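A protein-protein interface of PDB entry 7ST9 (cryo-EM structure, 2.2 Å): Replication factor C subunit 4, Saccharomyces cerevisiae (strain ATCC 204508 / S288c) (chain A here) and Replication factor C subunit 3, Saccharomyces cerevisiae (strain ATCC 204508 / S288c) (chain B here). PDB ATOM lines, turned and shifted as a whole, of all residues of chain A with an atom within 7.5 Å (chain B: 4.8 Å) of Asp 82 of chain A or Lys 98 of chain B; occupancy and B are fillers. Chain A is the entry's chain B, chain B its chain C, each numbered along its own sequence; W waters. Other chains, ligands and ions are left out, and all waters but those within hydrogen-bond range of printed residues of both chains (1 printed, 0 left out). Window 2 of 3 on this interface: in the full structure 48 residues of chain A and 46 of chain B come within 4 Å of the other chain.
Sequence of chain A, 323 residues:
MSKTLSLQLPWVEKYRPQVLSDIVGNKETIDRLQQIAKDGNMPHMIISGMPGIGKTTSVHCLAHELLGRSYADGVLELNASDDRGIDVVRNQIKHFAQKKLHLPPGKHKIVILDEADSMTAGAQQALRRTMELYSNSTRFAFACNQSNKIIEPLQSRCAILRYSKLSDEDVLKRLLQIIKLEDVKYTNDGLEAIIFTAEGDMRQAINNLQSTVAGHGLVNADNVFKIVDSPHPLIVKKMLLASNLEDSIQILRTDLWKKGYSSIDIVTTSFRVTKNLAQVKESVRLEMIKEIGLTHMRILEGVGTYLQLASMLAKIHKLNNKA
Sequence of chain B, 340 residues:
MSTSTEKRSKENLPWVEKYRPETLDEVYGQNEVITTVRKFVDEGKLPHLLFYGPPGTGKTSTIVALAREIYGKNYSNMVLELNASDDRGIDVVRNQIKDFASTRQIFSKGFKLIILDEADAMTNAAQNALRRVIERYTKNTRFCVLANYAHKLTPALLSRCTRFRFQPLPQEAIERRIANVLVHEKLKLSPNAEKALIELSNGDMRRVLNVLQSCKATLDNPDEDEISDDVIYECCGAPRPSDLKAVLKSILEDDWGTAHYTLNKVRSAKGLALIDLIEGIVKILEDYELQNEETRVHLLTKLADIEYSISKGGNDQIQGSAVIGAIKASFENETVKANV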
ATOM      1  N   GLU A  77     -16.238 -31.896  11.807  1.00  0.00           N
ATOM      2  CA  GLU A  77     -16.483 -30.850  10.822  1.00  0.00           C
ATOM      3  C   GLU A  77     -17.632 -29.964  11.283  1.00  0.00           C
ATOM      4  O   GLU A  77     -18.690 -30.467  11.675  1.00  0.00           O
ATOM      5  CB  GLU A  77     -16.803 -31.457   9.454  1.00  0.00           C
ATOM      6  CG  GLU A  77     -16.490 -30.542   8.281  1.00  0.00           C
ATOM      7  CD  GLU A  77     -17.478 -29.401   8.149  1.00  0.00           C
ATOM      8  OE1 GLU A  77     -18.698 -29.655   8.229  1.00  0.00           O
ATOM      9  OE2 GLU A  77     -17.034 -28.247   7.970  1.00  0.00           O
ATOM     10  N   LEU A  78     -17.418 -28.650  11.237  1.00  0.00           N
ATOM     11  CA  LEU A  78     -18.449 -27.677  11.560  1.00  0.00           C
ATOM     12  C   LEU A  78     -18.360 -26.517  10.580  1.00  0.00           C
ATOM     13  O   LEU A  78     -17.260 -26.094  10.212  1.00  0.00           O
ATOM     14  CB  LEU A  78     -18.309 -27.161  13.000  1.00  0.00           C
ATOM     15  CG  LEU A  78     -18.498 -28.200  14.106  1.00  0.00           C
ATOM     16  CD1 LEU A  78     -18.114 -27.616  15.457  1.00  0.00           C
ATOM     17  CD2 LEU A  78     -19.929 -28.714  14.130  1.00  0.00           C
ATOM     18  N   ASN A  79     -19.517 -26.006  10.166  1.00  0.00           N
ATOM     19  CA  ASN A  79     -19.587 -24.903   9.220  1.00  0.00           C
ATOM     20  C   ASN A  79     -20.678 -23.936   9.663  1.00  0.00           C
ATOM     21  O   ASN A  79     -21.309 -24.112  10.709  1.00  0.00           O
ATOM     22  CB  ASN A  79     -19.836 -25.413   7.796  1.00  0.00           C
ATOM     23  CG  ASN A  79     -21.090 -26.260   7.687  1.00  0.00           C
ATOM     24  OD1 ASN A  79     -22.201 -25.775   7.897  1.00  0.00           O
ATOM     25  ND2 ASN A  79     -20.916 -27.532   7.354  1.00  0.00           N
ATOM     26  N   ALA A  80     -20.900 -22.902   8.847  1.00  0.00           N
ATOM     27  CA  ALA A  80     -21.839 -21.847   9.208  1.00  0.00           C
ATOM     28  C   ALA A  80     -23.275 -22.347   9.309  1.00  0.00           C
ATOM     29  O   ALA A  80     -24.107 -21.678   9.931  1.00  0.00           O
ATOM     30  CB  ALA A  80     -21.760 -20.708   8.191  1.00  0.00           C
ATOM     31  N   SER A  81     -23.590 -23.498   8.714  1.00  0.00           N
ATOM     32  CA  SER A  81     -24.943 -24.036   8.787  1.00  0.00           C
ATOM     33  C   SER A  81     -25.213 -24.794  10.080  1.00  0.00           C
ATOM     34  O   SER A  81     -26.367 -25.148  10.341  1.00  0.00           O
ATOM     35  CB  SER A  81     -25.208 -24.957   7.592  1.00  0.00           C
ATOM     36  OG  SER A  81     -24.702 -26.259   7.825  1.00  0.00           O
ATOM     37  N   ASP A  82     -24.190 -25.050  10.888  1.00  0.00           N
ATOM     38  CA  ASP A  82     -24.340 -25.714  12.173  1.00  0.00           C
ATOM     39  C   ASP A  82     -24.262 -24.696  13.306  1.00  0.00           C
ATOM     40  O   ASP A  82     -23.809 -23.564  13.126  1.00  0.00           O
ATOM     41  CB  ASP A  82     -23.259 -26.781  12.366  1.00  0.00           C
ATOM     42  CG  ASP A  82     -23.248 -27.811  11.254  1.00  0.00           C
ATOM     43  OD1 ASP A  82     -24.305 -28.430  11.003  1.00  0.00           O
ATOM     44  OD2 ASP A  82     -22.183 -28.002  10.632  1.00  0.00           O
ATOM     45  N   ASP A  83     -24.714 -25.118  14.484  1.00  0.00           N
ATOM     46  CA  ASP A  83     -24.545 -24.303  15.678  1.00  0.00           C
ATOM     47  C   ASP A  83     -23.070 -24.252  16.052  1.00  0.00           C
ATOM     48  O   ASP A  83     -22.425 -25.292  16.214  1.00  0.00           O
ATOM     49  CB  ASP A  83     -25.371 -24.871  16.832  1.00  0.00           C
ATOM     50  CG  ASP A  83     -25.384 -23.958  18.047  1.00  0.00           C
ATOM     51  OD1 ASP A  83     -24.884 -22.818  17.946  1.00  0.00           O
ATOM     52  OD2 ASP A  83     -25.897 -24.382  19.103  1.00  0.00           O
ATOM     53  N   ARG A  84     -22.533 -23.038  16.183  1.00  0.00           N
ATOM     54  CA  ARG A  84     -21.116 -22.855  16.478  1.00  0.00           C
ATOM     55  C   ARG A  84     -20.897 -21.756  17.511  1.00  0.00           C
ATOM     56  O   ARG A  84     -19.875 -21.063  17.476  1.00  0.00           O
ATOM     57  CB  ARG A  84     -20.331 -22.533  15.204  1.00  0.00           C
ATOM     58  CG  ARG A  84     -20.358 -23.639  14.166  1.00  0.00           C
ATOM     59  CD  ARG A  84     -19.275 -23.445  13.117  1.00  0.00           C
ATOM     60  NE  ARG A  84     -19.425 -22.185  12.401  1.00  0.00           N
ATOM     61  CZ  ARG A  84     -18.684 -21.819  11.363  1.00  0.00           C
ATOM     62  NH1 ARG A  84     -17.724 -22.596  10.891  1.00  0.00           N
ATOM     63  NH2 ARG A  84     -18.914 -20.644  10.784  1.00  0.00           N
ATOM     64  N   GLY A  85     -21.838 -21.586  18.435  1.00  0.00           N
ATOM     65  CA  GLY A  85     -21.731 -20.567  19.454  1.00  0.00           C
ATOM     66  C   GLY A  85     -20.734 -20.945  20.534  1.00  0.00           C
ATOM     67  O   GLY A  85     -20.023 -21.947  20.456  1.00  0.00           O
ATOM     68  N   VAL A  88     -21.185 -24.348  22.066  1.00  0.00           N
ATOM     69  CA  VAL A  88     -20.658 -25.436  21.250  1.00  0.00           C
ATOM     70  C   VAL A  88     -19.165 -25.607  21.500  1.00  0.00           C
ATOM     71  O   VAL A  88     -18.681 -26.726  21.690  1.00  0.00           O
ATOM     72  CB  VAL A  88     -20.964 -25.187  19.762  1.00  0.00           C
ATOM     73  CG1 VAL A  88     -20.315 -26.257  18.895  1.00  0.00           C
ATOM     74  CG2 VAL A  88     -22.469 -25.150  19.537  1.00  0.00           C
ATOM     75  N   GLN A  92     -19.009 -29.369  22.772  1.00  0.00           N
ATOM     76  CA  GLN A  92     -18.788 -30.368  21.730  1.00  0.00           C
ATOM     77  C   GLN A  92     -17.326 -30.404  21.299  1.00  0.00           C
ATOM     78  O   GLN A  92     -16.698 -31.470  21.280  1.00  0.00           O
ATOM     79  CB  GLN A  92     -19.693 -30.080  20.531  1.00  0.00           C
ATOM     80  CG  GLN A  92     -19.762 -31.214  19.521  1.00  0.00           C
ATOM     81  CD  GLN A  92     -20.544 -30.841  18.276  1.00  0.00           C
ATOM     82  OE1 GLN A  92     -21.172 -29.785  18.218  1.00  0.00           O
ATOM     83  NE2 GLN A  92     -20.508 -31.708  17.272  1.00  0.00           N
ATOM     84  N   GLU A 115     -15.732 -21.948   6.773  1.00  0.00           N
ATOM     85  CA  GLU A 115     -16.290 -20.606   6.921  1.00  0.00           C
ATOM     86  C   GLU A 115     -16.056 -20.077   8.335  1.00  0.00           C
ATOM     87  O   GLU A 115     -16.934 -19.461   8.941  1.00  0.00           O
ATOM     88  CB  GLU A 115     -17.780 -20.590   6.575  1.00  0.00           C
ATOM     89  CG  GLU A 115     -18.076 -20.952   5.128  1.00  0.00           C
ATOM     90  CD  GLU A 115     -19.062 -22.099   4.994  1.00  0.00           C
ATOM     91  OE1 GLU A 115     -19.910 -22.274   5.894  1.00  0.00           O
ATOM     92  OE2 GLU A 115     -18.986 -22.827   3.983  1.00  0.00           O
ATOM     93  N   VAL B  93     -32.815 -20.577   8.447  1.00  0.00           N
ATOM     94  CA  VAL B  93     -31.967 -21.393   7.582  1.00  0.00           C
ATOM     95  C   VAL B  93     -31.493 -22.636   8.323  1.00  0.00           C
ATOM     96  O   VAL B  93     -31.513 -23.747   7.782  1.00  0.00           O
ATOM     97  CB  VAL B  93     -30.778 -20.561   7.063  1.00  0.00           C
ATOM     98  CG1 VAL B  93     -29.746 -21.459   6.390  1.00  0.00           C
ATOM     99  CG2 VAL B  93     -31.259 -19.484   6.107  1.00  0.00           C
ATOM    100  N   ARG B  94     -31.061 -22.466   9.574  1.00  0.00           N
ATOM    101  CA  ARG B  94     -30.529 -23.590  10.335  1.00  0.00           C
ATOM    102  C   ARG B  94     -31.598 -24.642  10.605  1.00  0.00           C
ATOM    103  O   ARG B  94     -31.318 -25.843  10.541  1.00  0.00           O
ATOM    104  CB  ARG B  94     -29.927 -23.093  11.651  1.00  0.00           C
ATOM    105  CG  ARG B  94     -28.550 -22.458  11.508  1.00  0.00           C
ATOM    106  CD  ARG B  94     -27.817 -22.410  12.844  1.00  0.00           C
ATOM    107  NE  ARG B  94     -28.512 -21.579  13.822  1.00  0.00           N
ATOM    108  CZ  ARG B  94     -28.146 -20.353  14.179  1.00  0.00           C
ATOM    109  NH1 ARG B  94     -27.080 -19.764  13.662  1.00  0.00           N
ATOM    110  NH2 ARG B  94     -28.872 -19.700  15.082  1.00  0.00           N
ATOM    111  N   ASN B  95     -32.822 -24.218  10.924  1.00  0.00           N
ATOM    112  CA  ASN B  95     -33.844 -25.184  11.315  1.00  0.00           C
ATOM    113  C   ASN B  95     -34.737 -25.613  10.156  1.00  0.00           C
ATOM    114  O   ASN B  95     -34.667 -26.763   9.715  1.00  0.00           O
ATOM    115  CB  ASN B  95     -34.703 -24.603  12.440  1.00  0.00           C
ATOM    116  CG  ASN B  95     -33.879 -24.142  13.626  1.00  0.00           C
ATOM    117  OD1 ASN B  95     -34.082 -23.048  14.150  1.00  0.00           O
ATOM    118  ND2 ASN B  95     -32.940 -24.977  14.055  1.00  0.00           N
ATOM    119  N   GLN B  96     -35.522 -24.689   9.602  1.00  0.00           N
ATOM    120  CA  GLN B  96     -36.583 -25.085   8.680  1.00  0.00           C
ATOM    121  C   GLN B  96     -36.013 -25.558   7.348  1.00  0.00           C
ATOM    122  O   GLN B  96     -36.313 -26.667   6.888  1.00  0.00           O
ATOM    123  CB  GLN B  96     -37.549 -23.917   8.469  1.00  0.00           C
ATOM    124  CG  GLN B  96     -38.598 -24.157   7.393  1.00  0.00           C
ATOM    125  CD  GLN B  96     -39.655 -23.070   7.355  1.00  0.00           C
ATOM    126  OE1 GLN B  96     -39.504 -22.020   7.981  1.00  0.00           O
ATOM    127  NE2 GLN B  96     -40.729 -23.314   6.615  1.00  0.00           N
ATOM    128  N   ILE B  97     -35.190 -24.722   6.712  1.00  0.00           N
ATOM    129  CA  ILE B  97     -34.629 -25.075   5.413  1.00  0.00           C
ATOM    130  C   ILE B  97     -33.758 -26.317   5.535  1.00  0.00           C
ATOM    131  O   ILE B  97     -33.813 -27.218   4.690  1.00  0.00           O
ATOM    132  CB  ILE B  97     -33.845 -23.883   4.830  1.00  0.00           C
ATOM    133  CG1 ILE B  97     -34.813 -22.772   4.413  1.00  0.00           C
ATOM    134  CG2 ILE B  97     -32.995 -24.329   3.648  1.00  0.00           C
ATOM    135  CD1 ILE B  97     -34.155 -21.426   4.192  1.00  0.00           C
ATOM    136  N   LYS B  98     -32.941 -26.387   6.587  1.00  0.00           N
ATOM    137  CA  LYS B  98     -32.060 -27.534   6.764  1.00  0.00           C
ATOM    138  C   LYS B  98     -32.858 -28.821   6.949  1.00  0.00           C
ATOM    139  O   LYS B  98     -32.547 -29.848   6.336  1.00  0.00           O
ATOM    140  CB  LYS B  98     -31.131 -27.300   7.956  1.00  0.00           C
ATOM    141  CG  LYS B  98     -29.943 -28.245   8.010  1.00  0.00           C
ATOM    142  CD  LYS B  98     -28.970 -27.850   9.108  1.00  0.00           C
ATOM    143  CE  LYS B  98     -27.940 -28.939   9.358  1.00  0.00           C
ATOM    144  NZ  LYS B  98     -26.557 -28.395   9.432  1.00  0.00           N
ATOM    145  N   ASP B  99     -33.898 -28.787   7.789  1.00  0.00           N
ATOM    146  CA  ASP B  99     -34.696 -29.989   8.010  1.00  0.00           C
ATOM    147  C   ASP B  99     -35.421 -30.412   6.740  1.00  0.00           C
ATOM    148  O   ASP B  99     -35.501 -31.607   6.435  1.00  0.00           O
ATOM    149  CB  ASP B  99     -35.691 -29.761   9.149  1.00  0.00           C
ATOM    150  CG  ASP B  99     -35.008 -29.427  10.464  1.00  0.00           C
ATOM    151  OD1 ASP B  99     -33.915 -29.974  10.724  1.00  0.00           O
ATOM    152  OD2 ASP B  99     -35.567 -28.624  11.241  1.00  0.00           O
ATOM    153  N   PHE B 100     -35.963 -29.453   5.985  1.00  0.00           N
ATOM    154  CA  PHE B 100     -36.633 -29.810   4.739  1.00  0.00           C
ATOM    155  C   PHE B 100     -35.652 -30.410   3.738  1.00  0.00           C
ATOM    156  O   PHE B 100     -35.973 -31.388   3.052  1.00  0.00           O
ATOM    157  CB  PHE B 100     -37.325 -28.589   4.135  1.00  0.00           C
ATOM    158  CG  PHE B 100     -38.043 -28.881   2.848  1.00  0.00           C
ATOM    159  CD1 PHE B 100     -39.315 -29.427   2.857  1.00  0.00           C
ATOM    160  CD2 PHE B 100     -37.442 -28.619   1.629  1.00  0.00           C
ATOM    161  CE1 PHE B 100     -39.977 -29.699   1.675  1.00  0.00           C
ATOM    162  CE2 PHE B 100     -38.099 -28.889   0.442  1.00  0.00           C
ATOM    163  CZ  PHE B 100     -39.368 -29.430   0.466  1.00  0.00           C
ATOM    164  N   ALA B 101     -34.449 -29.839   3.639  1.00  0.00           N
ATOM    165  CA  ALA B 101     -33.480 -30.311   2.658  1.00  0.00           C
ATOM    166  C   ALA B 101     -32.864 -31.649   3.040  1.00  0.00           C
ATOM    167  O   ALA B 101     -32.364 -32.359   2.159  1.00  0.00           O
ATOM    168  CB  ALA B 101     -32.374 -29.272   2.470  1.00  0.00           C
ATOM    169  N   SER B 102     -32.888 -32.013   4.321  1.00  0.00           N
ATOM    170  CA  SER B 102     -32.253 -33.231   4.804  1.00  0.00           C
ATOM    171  C   SER B 102     -33.242 -34.373   5.015  1.00  0.00           C
ATOM    172  O   SER B 102     -32.866 -35.405   5.578  1.00  0.00           O
ATOM    173  CB  SER B 102     -31.505 -32.947   6.108  1.00  0.00           C
ATOM    174  OG  SER B 102     -32.404 -32.619   7.152  1.00  0.00           O
ATOM    175  N   VAL B 133     -25.478 -25.947   3.371  1.00  0.00           N
ATOM    176  CA  VAL B 133     -26.761 -26.615   3.176  1.00  0.00           C
ATOM    177  C   VAL B 133     -26.958 -26.945   1.703  1.00  0.00           C
ATOM    178  O   VAL B 133     -27.370 -28.055   1.347  1.00  0.00           O
ATOM    179  CB  VAL B 133     -27.911 -25.747   3.719  1.00  0.00           C
ATOM    180  CG1 VAL B 133     -29.250 -26.434   3.489  1.00  0.00           C
ATOM    181  CG2 VAL B 133     -27.703 -25.451   5.195  1.00  0.00           C
ATOM    182  N   ARG B 136     -24.078 -29.778   0.735  1.00  0.00           N
ATOM    183  CA  ARG B 136     -24.149 -31.110   1.329  1.00  0.00           C
ATOM    184  C   ARG B 136     -25.320 -31.917   0.776  1.00  0.00           C
ATOM    185  O   ARG B 136     -25.169 -33.107   0.475  1.00  0.00           O
ATOM    186  CB  ARG B 136     -24.256 -30.995   2.849  1.00  0.00           C
ATOM    187  CG  ARG B 136     -24.423 -32.330   3.558  1.00  0.00           C
ATOM    188  CD  ARG B 136     -24.052 -32.238   5.028  1.00  0.00           C
ATOM    189  NE  ARG B 136     -25.054 -31.515   5.804  1.00  0.00           N
ATOM    190  CZ  ARG B 136     -25.003 -30.220   6.090  1.00  0.00           C
ATOM    191  NH1 ARG B 136     -24.005 -29.456   5.675  1.00  0.00           N
ATOM    192  NH2 ARG B 136     -25.980 -29.677   6.810  1.00  0.00           N
ATOM    193  N   TYR B 137     -26.490 -31.296   0.636  1.00  0.00           N
ATOM    194  CA  TYR B 137     -27.714 -32.000   0.270  1.00  0.00           C
ATOM    195  C   TYR B 137     -28.072 -31.825  -1.202  1.00  0.00           C
ATOM    196  O   TYR B 137     -29.256 -31.806  -1.555  1.00  0.00           O
ATOM    197  CB  TYR B 137     -28.868 -31.534   1.158  1.00  0.00           C
ATOM    198  CG  TYR B 137     -28.616 -31.743   2.633  1.00  0.00           C
ATOM    199  CD1 TYR B 137     -28.605 -33.019   3.180  1.00  0.00           C
ATOM    200  CD2 TYR B 137     -28.383 -30.668   3.478  1.00  0.00           C
ATOM    201  CE1 TYR B 137     -28.372 -33.217   4.526  1.00  0.00           C
ATOM    202  CE2 TYR B 137     -28.149 -30.855   4.826  1.00  0.00           C
ATOM    203  CZ  TYR B 137     -28.144 -32.132   5.344  1.00  0.00           C
ATOM    204  OH  TYR B 137     -27.913 -32.324   6.686  1.00  0.00           O
HETATM  205  O   HOH W   1     -24.618 -21.211  12.649  1.00  0.00           O
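O of Ser 81 of chain A touches CG of Arg 94 of chain B, 3.7 Å away.
CB of Ser 81 of chain A touches CG2 of Val 133 of chain B (3.5 Å).
Ser 81 of chain A touches Arg 136 of chain B.
Water W1 lies within hydrogen-bond range of O of Asp 82 of chain A (2.5 Å), O of Ala 80 of chain A (2.8 Å) and NH1 of Arg 94 of chain B (3.0 Å).
The side-chain carboxylate (OD1) of Asp 82 of chain A is in salt-bridge range of the side-chain amino group (NZ) of Lys 98 of chain B.
The side-chain hydroxyl of Ser 81 of chain A sits at hydrogen-bond distance from the side-chain amino group of Lys 98 of chain B (3.3 Å).
Printed residues of chain B that touch a printed residue of chain A: Arg 94, Lys 98, Val 133 and Arg 136.
Among the printed residues, Asp or Glu carboxylates within 4 Å of a Lys or Arg side-chain nitrogen of the other chain: Asp 82 of chain A with Lys 98 of chain B.
O of Lys 98 of chain B is in hydrogen-bond range of OG of Ser 102 of chain B (2.9 Å).
The backbone NH (N) of Lys 98 of chain B sits at hydrogen-bond distance from the backbone carbonyl oxygen (O) of Val 93 of chain B (3.2 Å).
The backbone NH (N) of Asn 79 of chain A lies within hydrogen-bond range of the side-chain carboxylate (OD2) of Asp 82 of chain A (3.4 Å).
NE of Arg 136 of chain B is in hydrogen-bond range of OH of Tyr 137 of chain B (3.1 Å).
The side-chain amide oxygen (OD1) of Asn 79 of chain A lies within hydrogen-bond range of the side-chain hydroxyl (OG) of Ser 81 of chain A (2.5 Å).
Of chain A, only Ser 81 and Asp 82 come within 4 Å of Lys 98 of chain B.
Of the printed residues of chain A, Arg 136 of chain B touches Ser 81 (3.8 Å).
Of the printed residues of chain A, Arg 94 of chain B touches Ser 81.
Asp 99 of chain B touches none of the printed residues of chain A.
Gly 85 of chain A touches none of the printed residues of chain B.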
